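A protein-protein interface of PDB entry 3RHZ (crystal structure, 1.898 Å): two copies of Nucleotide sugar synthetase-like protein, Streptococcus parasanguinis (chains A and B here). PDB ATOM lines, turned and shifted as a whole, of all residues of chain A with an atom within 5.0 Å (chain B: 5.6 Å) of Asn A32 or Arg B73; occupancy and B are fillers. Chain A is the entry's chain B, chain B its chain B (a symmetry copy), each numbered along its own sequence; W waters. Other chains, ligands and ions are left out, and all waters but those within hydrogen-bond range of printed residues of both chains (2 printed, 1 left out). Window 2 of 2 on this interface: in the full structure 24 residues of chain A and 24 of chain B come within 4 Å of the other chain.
OD1 of Asn A17 sits at hydrogen-bond distance from ND2 of Asn A32. OD1 of Asn A17 lies close to OG1 of Thr A35 (3.2 Å). The side-chain hydroxyl of Thr A35 lies within hydrogen-bond range of the backbone carbonyl oxygen of Gln A31 (2.9 Å). The backbone carbonyl oxygen (O) of Gly B71 is in hydrogen-bond range of the guanidinium group (NH2) of Arg B12 (2.9 Å). The side-chain hydroxyl (OH) of Tyr B14 sits at hydrogen-bond distance from the backbone carbonyl oxygen (O) of Gly B71 (3.3 Å). The backbone NH (N) of Arg B73 lies within hydrogen-bond range of the side-chain carboxylate (OD2) of Asp B76, at 2.9 Å.
Water W1 lies within hydrogen-bond range of the side-chain carboxylate (OD1) of Asp A36, the guanidinium group (NH1) of Arg B44, the side-chain amide nitrogen (ND2) of Asn A17 and the backbone carbonyl oxygen (O) of Asn A32. Water W2 bridges NH1 of Arg B12 and OD1 of Asp A36.
Among the printed residues, pairs that only touch across the chains: Asn A19 with Gly B71 and Thr A35 with Arg B44.
Of the printed residues of chain B, Asn A32 touches Arg B73 (2.6 Å). Arg B73 touches just these residues of chain A: Asn A19, Gln A28 and Asn A32. Printed residues of chain B within 4 Å of Asp A36: Arg B44. Of the printed residues of chain A, Arg B44 touches Thr A35 (3.8 Å) and Asp A36 (2.8 Å). The nearest residue of chain A that does not touch Arg B73 is Ile A18 (4.6 Å). The nearest printed residue of chain A that does not touch Arg B44 is Asn A17 (4.2 Å).
The side-chain amide oxygen of Asn A19 sits close to the backbone carbonyl oxygen of Leu B72, at 3.0 Å. ND2 of Asn A19 lies close to NE of Arg B73 (3.0 Å). The side-chain amide oxygen (OE1) of Gln A28 is in hydrogen-bond range of the guanidinium group (NH2) of Arg B73 (2.9 Å). OD1 of Asn A32 is in hydrogen-bond range of NH2 of Arg B73 (2.6 Å). The side-chain carboxylate (OD1) of Asp A36 lies within salt-bridge range of the guanidinium group (NH2) of Arg B44.
Of the 12 printed residues of chain A, 5 touch a printed residue of chain B. Along chain A the printed residues that touch a printed residue of chain B span positions 19 to 36.
No position is printed for both chains.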
ATOM      1  N   ASN A  17     -26.675  -2.283 -33.343  1.00  0.00           N
ATOM      2  CA  ASN A  17     -25.721  -1.194 -33.482  1.00  0.00           C
ATOM      3  C   ASN A  17     -24.328  -1.666 -33.113  1.00  0.00           C
ATOM      4  O   ASN A  17     -24.107  -2.116 -31.985  1.00  0.00           O
ATOM      5  CB  ASN A  17     -26.151  -0.051 -32.559  1.00  0.00           C
ATOM      6  CG  ASN A  17     -25.306   1.188 -32.733  1.00  0.00           C
ATOM      7  OD1 ASN A  17     -24.892   1.526 -33.849  1.00  0.00           O
ATOM      8  ND2 ASN A  17     -25.062   1.889 -31.633  1.00  0.00           N
ATOM      9  N   ILE A  18     -23.393  -1.587 -34.059  1.00  0.00           N
ATOM     10  CA  ILE A  18     -22.037  -2.078 -33.796  1.00  0.00           C
ATOM     11  C   ILE A  18     -21.177  -1.114 -32.981  1.00  0.00           C
ATOM     12  O   ILE A  18     -21.457   0.091 -32.901  1.00  0.00           O
ATOM     13  CB  ILE A  18     -21.305  -2.506 -35.069  1.00  0.00           C
ATOM     14  CG1 ILE A  18     -21.136  -1.321 -36.033  1.00  0.00           C
ATOM     15  CG2 ILE A  18     -22.020  -3.688 -35.728  1.00  0.00           C
ATOM     16  CD1 ILE A  18     -20.307  -1.709 -37.262  1.00  0.00           C
ATOM     17  N   ASN A  19     -20.138  -1.663 -32.364  1.00  0.00           N
ATOM     18  CA  ASN A  19     -19.273  -0.930 -31.454  1.00  0.00           C
ATOM     19  C   ASN A  19     -17.915  -1.619 -31.530  1.00  0.00           C
ATOM     20  O   ASN A  19     -17.851  -2.798 -31.870  1.00  0.00           O
ATOM     21  CB  ASN A  19     -19.885  -0.980 -30.034  1.00  0.00           C
ATOM     22  CG  ASN A  19     -19.116  -0.144 -29.023  1.00  0.00           C
ATOM     23  OD1 ASN A  19     -19.089  -0.458 -27.827  1.00  0.00           O
ATOM     24  ND2 ASN A  19     -18.492   0.928 -29.494  1.00  0.00           N
ATOM     25  N   GLN A  28     -19.271   1.879 -38.955  1.00  0.00           N
ATOM     26  CA  GLN A  28     -19.738   2.121 -37.592  1.00  0.00           C
ATOM     27  C   GLN A  28     -20.380   3.503 -37.455  1.00  0.00           C
ATOM     28  O   GLN A  28     -21.356   3.663 -36.756  1.00  0.00           O
ATOM     29  CB  GLN A  28     -18.622   1.947 -36.564  1.00  0.00           C
ATOM     30  CG  GLN A  28     -19.135   2.184 -35.148  1.00  0.00           C
ATOM     31  CD  GLN A  28     -18.119   1.843 -34.072  1.00  0.00           C
ATOM     32  OE1 GLN A  28     -17.885   2.626 -33.154  1.00  0.00           O
ATOM     33  NE2 GLN A  28     -17.536   0.664 -34.163  1.00  0.00           N
ATOM     34  N   LEU A  29     -19.830   4.502 -38.132  1.00  0.00           N
ATOM     35  CA  LEU A  29     -20.428   5.841 -38.085  1.00  0.00           C
ATOM     36  C   LEU A  29     -21.894   5.809 -38.517  1.00  0.00           C
ATOM     37  O   LEU A  29     -22.768   6.388 -37.844  1.00  0.00           O
ATOM     38  CB  LEU A  29     -19.646   6.816 -38.982  1.00  0.00           C
ATOM     39  CG  LEU A  29     -19.230   8.145 -38.364  1.00  0.00           C
ATOM     40  CD1 LEU A  29     -20.442   8.883 -37.827  1.00  0.00           C
ATOM     41  CD2 LEU A  29     -18.206   7.914 -37.264  1.00  0.00           C
ATOM     42  N   CYS A  30     -22.166   5.166 -39.653  1.00  0.00           N
ATOM     43  CA  CYS A  30     -23.543   5.070 -40.155  1.00  0.00           C
ATOM     44  C   CYS A  30     -24.461   4.344 -39.194  1.00  0.00           C
ATOM     45  O   CYS A  30     -25.576   4.810 -38.922  1.00  0.00           O
ATOM     46  CB  CYS A  30     -23.606   4.380 -41.513  1.00  0.00           C
ATOM     47  SG  CYS A  30     -22.959   5.380 -42.843  1.00  0.00           S
ATOM     48  N   GLN A  31     -24.021   3.195 -38.681  1.00  0.00           N
ATOM     49  CA  GLN A  31     -24.861   2.495 -37.697  1.00  0.00           C
ATOM     50  C   GLN A  31     -25.117   3.336 -36.457  1.00  0.00           C
ATOM     51  O   GLN A  31     -26.235   3.366 -35.950  1.00  0.00           O
ATOM     52  CB  GLN A  31     -24.286   1.117 -37.302  1.00  0.00           C
ATOM     53  CG  GLN A  31     -24.288   0.106 -38.440  1.00  0.00           C
ATOM     54  CD  GLN A  31     -24.317  -1.340 -37.957  1.00  0.00           C
ATOM     55  OE1 GLN A  31     -24.650  -1.626 -36.805  1.00  0.00           O
ATOM     56  NE2 GLN A  31     -23.965  -2.252 -38.842  1.00  0.00           N
ATOM     57  N   ASN A  32     -24.087   3.993 -35.932  1.00  0.00           N
ATOM     58  CA  ASN A  32     -24.269   4.763 -34.704  1.00  0.00           C
ATOM     59  C   ASN A  32     -25.189   5.971 -34.936  1.00  0.00           C
ATOM     60  O   ASN A  32     -25.973   6.353 -34.073  1.00  0.00           O
ATOM     61  CB  ASN A  32     -22.924   5.255 -34.148  1.00  0.00           C
ATOM     62  CG  ASN A  32     -21.984   4.125 -33.731  1.00  0.00           C
ATOM     63  OD1 ASN A  32     -20.816   4.377 -33.459  1.00  0.00           O
ATOM     64  ND2 ASN A  32     -22.490   2.886 -33.669  1.00  0.00           N
ATOM     65  N   THR A  33     -25.064   6.585 -36.106  1.00  0.00           N
ATOM     66  CA  THR A  33     -25.894   7.747 -36.430  1.00  0.00           C
ATOM     67  C   THR A  33     -27.350   7.330 -36.553  1.00  0.00           C
ATOM     68  O   THR A  33     -28.237   7.985 -36.015  1.00  0.00           O
ATOM     69  CB  THR A  33     -25.433   8.417 -37.739  1.00  0.00           C
ATOM     70  OG1 THR A  33     -24.107   8.912 -37.554  1.00  0.00           O
ATOM     71  CG2 THR A  33     -26.351   9.586 -38.096  1.00  0.00           C
ATOM     72  N   VAL A  34     -27.590   6.216 -37.238  1.00  0.00           N
ATOM     73  CA  VAL A  34     -28.940   5.698 -37.359  1.00  0.00           C
ATOM     74  C   VAL A  34     -29.488   5.400 -35.973  1.00  0.00           C
ATOM     75  O   VAL A  34     -30.643   5.705 -35.677  1.00  0.00           O
ATOM     76  CB  VAL A  34     -28.987   4.432 -38.233  1.00  0.00           C
ATOM     77  CG1 VAL A  34     -30.364   3.787 -38.166  1.00  0.00           C
ATOM     78  CG2 VAL A  34     -28.638   4.769 -39.681  1.00  0.00           C
ATOM     79  N   THR A  35     -28.666   4.801 -35.117  1.00  0.00           N
ATOM     80  CA  THR A  35     -29.152   4.437 -33.790  1.00  0.00           C
ATOM     81  C   THR A  35     -29.467   5.677 -32.950  1.00  0.00           C
ATOM     82  O   THR A  35     -30.405   5.674 -32.159  1.00  0.00           O
ATOM     83  CB  THR A  35     -28.150   3.519 -33.061  1.00  0.00           C
ATOM     84  OG1 THR A  35     -27.968   2.322 -33.835  1.00  0.00           O
ATOM     85  CG2 THR A  35     -28.674   3.147 -31.684  1.00  0.00           C
ATOM     86  N   ASP A  36     -28.678   6.739 -33.122  1.00  0.00           N
ATOM     87  CA  ASP A  36     -28.941   7.961 -32.373  1.00  0.00           C
ATOM     88  C   ASP A  36     -30.330   8.480 -32.745  1.00  0.00           C
ATOM     89  O   ASP A  36     -31.096   8.909 -31.876  1.00  0.00           O
ATOM     90  CB  ASP A  36     -27.895   9.024 -32.671  1.00  0.00           C
ATOM     91  CG  ASP A  36     -26.556   8.728 -32.041  1.00  0.00           C
ATOM     92  OD1 ASP A  36     -26.456   7.770 -31.231  1.00  0.00           O
ATOM     93  OD2 ASP A  36     -25.596   9.467 -32.371  1.00  0.00           O
ATOM     94  N   ARG B  12     -23.283   8.691 -22.819  1.00  0.00           N
ATOM     95  CA  ARG B  12     -24.594   8.132 -23.278  1.00  0.00           C
ATOM     96  C   ARG B  12     -24.791   7.564 -21.832  1.00  0.00           C
ATOM     97  O   ARG B  12     -23.842   7.090 -21.161  1.00  0.00           O
ATOM     98  CB  ARG B  12     -24.540   6.956 -24.277  1.00  0.00           C
ATOM     99  CG  ARG B  12     -24.556   7.340 -25.767  1.00  0.00           C
ATOM    100  CD  ARG B  12     -23.149   7.314 -26.330  1.00  0.00           C
ATOM    101  NE  ARG B  12     -22.445   6.135 -25.837  1.00  0.00           N
ATOM    102  CZ  ARG B  12     -22.449   4.950 -26.441  1.00  0.00           C
ATOM    103  NH1 ARG B  12     -23.095   4.794 -27.596  1.00  0.00           N
ATOM    104  NH2 ARG B  12     -21.799   3.927 -25.886  1.00  0.00           N
ATOM    105  N   TYR B  14     -26.593   4.557 -19.748  1.00  0.00           N
ATOM    106  CA  TYR B  14     -27.221   3.246 -19.886  1.00  0.00           C
ATOM    107  C   TYR B  14     -27.864   2.847 -18.560  1.00  0.00           C
ATOM    108  O   TYR B  14     -27.436   3.287 -17.507  1.00  0.00           O
ATOM    109  CB  TYR B  14     -26.196   2.183 -20.293  1.00  0.00           C
ATOM    110  CG  TYR B  14     -25.884   2.177 -21.773  1.00  0.00           C
ATOM    111  CD1 TYR B  14     -24.941   3.054 -22.315  1.00  0.00           C
ATOM    112  CD2 TYR B  14     -26.514   1.280 -22.624  1.00  0.00           C
ATOM    113  CE1 TYR B  14     -24.653   3.049 -23.681  1.00  0.00           C
ATOM    114  CE2 TYR B  14     -26.224   1.249 -23.981  1.00  0.00           C
ATOM    115  CZ  TYR B  14     -25.296   2.138 -24.505  1.00  0.00           C
ATOM    116  OH  TYR B  14     -25.028   2.111 -25.859  1.00  0.00           O
ATOM    117  N   ARG B  44     -30.334   4.501 -22.408  1.00  0.00           N
ATOM    118  CA  ARG B  44     -30.331   3.269 -23.202  1.00  0.00           C
ATOM    119  C   ARG B  44     -30.352   2.044 -22.288  1.00  0.00           C
ATOM    120  O   ARG B  44     -29.679   2.020 -21.274  1.00  0.00           O
ATOM    121  CB  ARG B  44     -29.074   3.211 -24.078  1.00  0.00           C
ATOM    122  CG  ARG B  44     -28.923   4.428 -24.995  1.00  0.00           C
ATOM    123  CD  ARG B  44     -27.853   4.242 -26.066  1.00  0.00           C
ATOM    124  NE  ARG B  44     -27.835   5.409 -26.952  1.00  0.00           N
ATOM    125  CZ  ARG B  44     -27.305   5.434 -28.168  1.00  0.00           C
ATOM    126  NH1 ARG B  44     -26.696   4.361 -28.672  1.00  0.00           N
ATOM    127  NH2 ARG B  44     -27.369   6.554 -28.878  1.00  0.00           N
ATOM    128  N   GLY B  71     -22.475  -2.565 -26.075  1.00  0.00           N
ATOM    129  CA  GLY B  71     -22.651  -1.206 -26.584  1.00  0.00           C
ATOM    130  C   GLY B  71     -21.932  -0.139 -25.771  1.00  0.00           C
ATOM    131  O   GLY B  71     -21.877   1.020 -26.171  1.00  0.00           O
ATOM    132  N   LEU B  72     -21.373  -0.518 -24.624  1.00  0.00           N
ATOM    133  CA  LEU B  72     -20.793   0.472 -23.720  1.00  0.00           C
ATOM    134  C   LEU B  72     -19.482   1.020 -24.251  1.00  0.00           C
ATOM    135  O   LEU B  72     -18.771   0.332 -24.977  1.00  0.00           O
ATOM    136  CB  LEU B  72     -20.516  -0.134 -22.345  1.00  0.00           C
ATOM    137  CG  LEU B  72     -21.664  -0.336 -21.381  1.00  0.00           C
ATOM    138  CD1 LEU B  72     -21.051  -0.784 -20.057  1.00  0.00           C
ATOM    139  CD2 LEU B  72     -22.484   0.932 -21.220  1.00  0.00           C
ATOM    140  N   ARG B  73     -19.160   2.246 -23.851  1.00  0.00           N
ATOM    141  CA  ARG B  73     -17.899   2.874 -24.209  1.00  0.00           C
ATOM    142  C   ARG B  73     -17.355   3.640 -23.022  1.00  0.00           C
ATOM    143  O   ARG B  73     -18.112   4.088 -22.168  1.00  0.00           O
ATOM    144  CB  ARG B  73     -18.121   3.873 -25.334  1.00  0.00           C
ATOM    145  CG  ARG B  73     -18.522   3.262 -26.638  1.00  0.00           C
ATOM    146  CD  ARG B  73     -18.785   4.354 -27.655  1.00  0.00           C
ATOM    147  NE  ARG B  73     -19.032   3.790 -28.975  1.00  0.00           N
ATOM    148  CZ  ARG B  73     -19.434   4.500 -30.022  1.00  0.00           C
ATOM    149  NH1 ARG B  73     -19.624   5.810 -29.906  1.00  0.00           N
ATOM    150  NH2 ARG B  73     -19.638   3.899 -31.184  1.00  0.00           N
ATOM    151  N   HIS B  74     -16.041   3.820 -22.985  1.00  0.00           N
ATOM    152  CA  HIS B  74     -15.443   4.690 -21.992  1.00  0.00           C
ATOM    153  C   HIS B  74     -16.133   6.048 -22.077  1.00  0.00           C
ATOM    154  O   HIS B  74     -16.428   6.539 -23.170  1.00  0.00           O
ATOM    155  CB  HIS B  74     -13.949   4.850 -22.258  1.00  0.00           C
ATOM    156  CG  HIS B  74     -13.190   3.562 -22.230  1.00  0.00           C
ATOM    157  ND1 HIS B  74     -13.206   2.712 -21.147  1.00  0.00           N
ATOM    158  CD2 HIS B  74     -12.387   2.982 -23.155  1.00  0.00           C
ATOM    159  CE1 HIS B  74     -12.439   1.664 -21.401  1.00  0.00           C
ATOM    160  NE2 HIS B  74     -11.937   1.802 -22.611  1.00  0.00           N
ATOM    161  N   GLY B  75     -16.406   6.658 -20.932  1.00  0.00           N
ATOM    162  CA  GLY B  75     -17.026   7.976 -20.944  1.00  0.00           C
ATOM    163  C   GLY B  75     -18.530   7.941 -20.742  1.00  0.00           C
ATOM    164  O   GLY B  75     -19.151   8.981 -20.529  1.00  0.00           O
ATOM    165  N   ASP B  76     -19.123   6.750 -20.826  1.00  0.00           N
ATOM    166  CA  ASP B  76     -20.551   6.592 -20.548  1.00  0.00           C
ATOM    167  C   ASP B  76     -20.822   6.608 -19.043  1.00  0.00           C
ATOM    168  O   ASP B  76     -19.899   6.615 -18.212  1.00  0.00           O
ATOM    169  CB  ASP B  76     -21.101   5.276 -21.131  1.00  0.00           C
ATOM    170  CG  ASP B  76     -21.158   5.272 -22.652  1.00  0.00           C
ATOM    171  OD1 ASP B  76     -21.126   6.361 -23.276  1.00  0.00           O
ATOM    172  OD2 ASP B  76     -21.242   4.166 -23.233  1.00  0.00           O
ATOM    173  N   TYR B 101     -14.475  -0.545 -17.645  1.00  0.00           N
ATOM    174  CA  TYR B 101     -14.643   0.626 -18.495  1.00  0.00           C
ATOM    175  C   TYR B 101     -14.362   1.896 -17.706  1.00  0.00           C
ATOM    176  O   TYR B 101     -14.547   1.940 -16.495  1.00  0.00           O
ATOM    177  CB  TYR B 101     -16.068   0.694 -19.032  1.00  0.00           C
ATOM    178  CG  TYR B 101     -16.445  -0.427 -19.969  1.00  0.00           C
ATOM    179  CD1 TYR B 101     -16.827  -1.669 -19.480  1.00  0.00           C
ATOM    180  CD2 TYR B 101     -16.447  -0.232 -21.344  1.00  0.00           C
ATOM    181  CE1 TYR B 101     -17.183  -2.692 -20.344  1.00  0.00           C
ATOM    182  CE2 TYR B 101     -16.803  -1.240 -22.212  1.00  0.00           C
ATOM    183  CZ  TYR B 101     -17.173  -2.469 -21.709  1.00  0.00           C
ATOM    184  OH  TYR B 101     -17.529  -3.474 -22.583  1.00  0.00           O
ATOM    185  N   ASP B 102     -13.930   2.934 -18.405  1.00  0.00           N
ATOM    186  CA  ASP B 102     -13.731   4.226 -17.778  1.00  0.00           C
ATOM    187  C   ASP B 102     -15.077   4.958 -17.749  1.00  0.00           C
ATOM    188  O   ASP B 102     -15.325   5.863 -18.545  1.00  0.00           O
ATOM    189  CB  ASP B 102     -12.688   5.031 -18.551  1.00  0.00           C
ATOM    190  CG  ASP B 102     -12.405   6.378 -17.922  1.00  0.00           C
ATOM    191  OD1 ASP B 102     -12.660   6.535 -16.710  1.00  0.00           O
ATOM    192  OD2 ASP B 102     -11.922   7.279 -18.642  1.00  0.00           O
ATOM    193  N   ILE B 103     -15.942   4.531 -16.834  1.00  0.00           N
ATOM    194  CA  ILE B 103     -17.297   5.057 -16.725  1.00  0.00           C
ATOM    195  C   ILE B 103     -17.615   5.361 -15.271  1.00  0.00           C
ATOM    196  O   ILE B 103     -16.900   4.931 -14.360  1.00  0.00           O
ATOM    197  CB  ILE B 103     -18.325   4.045 -17.257  1.00  0.00           C
ATOM    198  CG1 ILE B 103     -18.220   2.727 -16.478  1.00  0.00           C
ATOM    199  CG2 ILE B 103     -18.108   3.802 -18.750  1.00  0.00           C
ATOM    200  CD1 ILE B 103     -19.309   1.729 -16.806  1.00  0.00           C
HETATM  201  O   HOH W   1     -25.390   4.986 -31.293  1.00  0.00           O
HETATM  202  O   HOH W   2     -23.708   6.956 -29.681  1.00  0.00           O
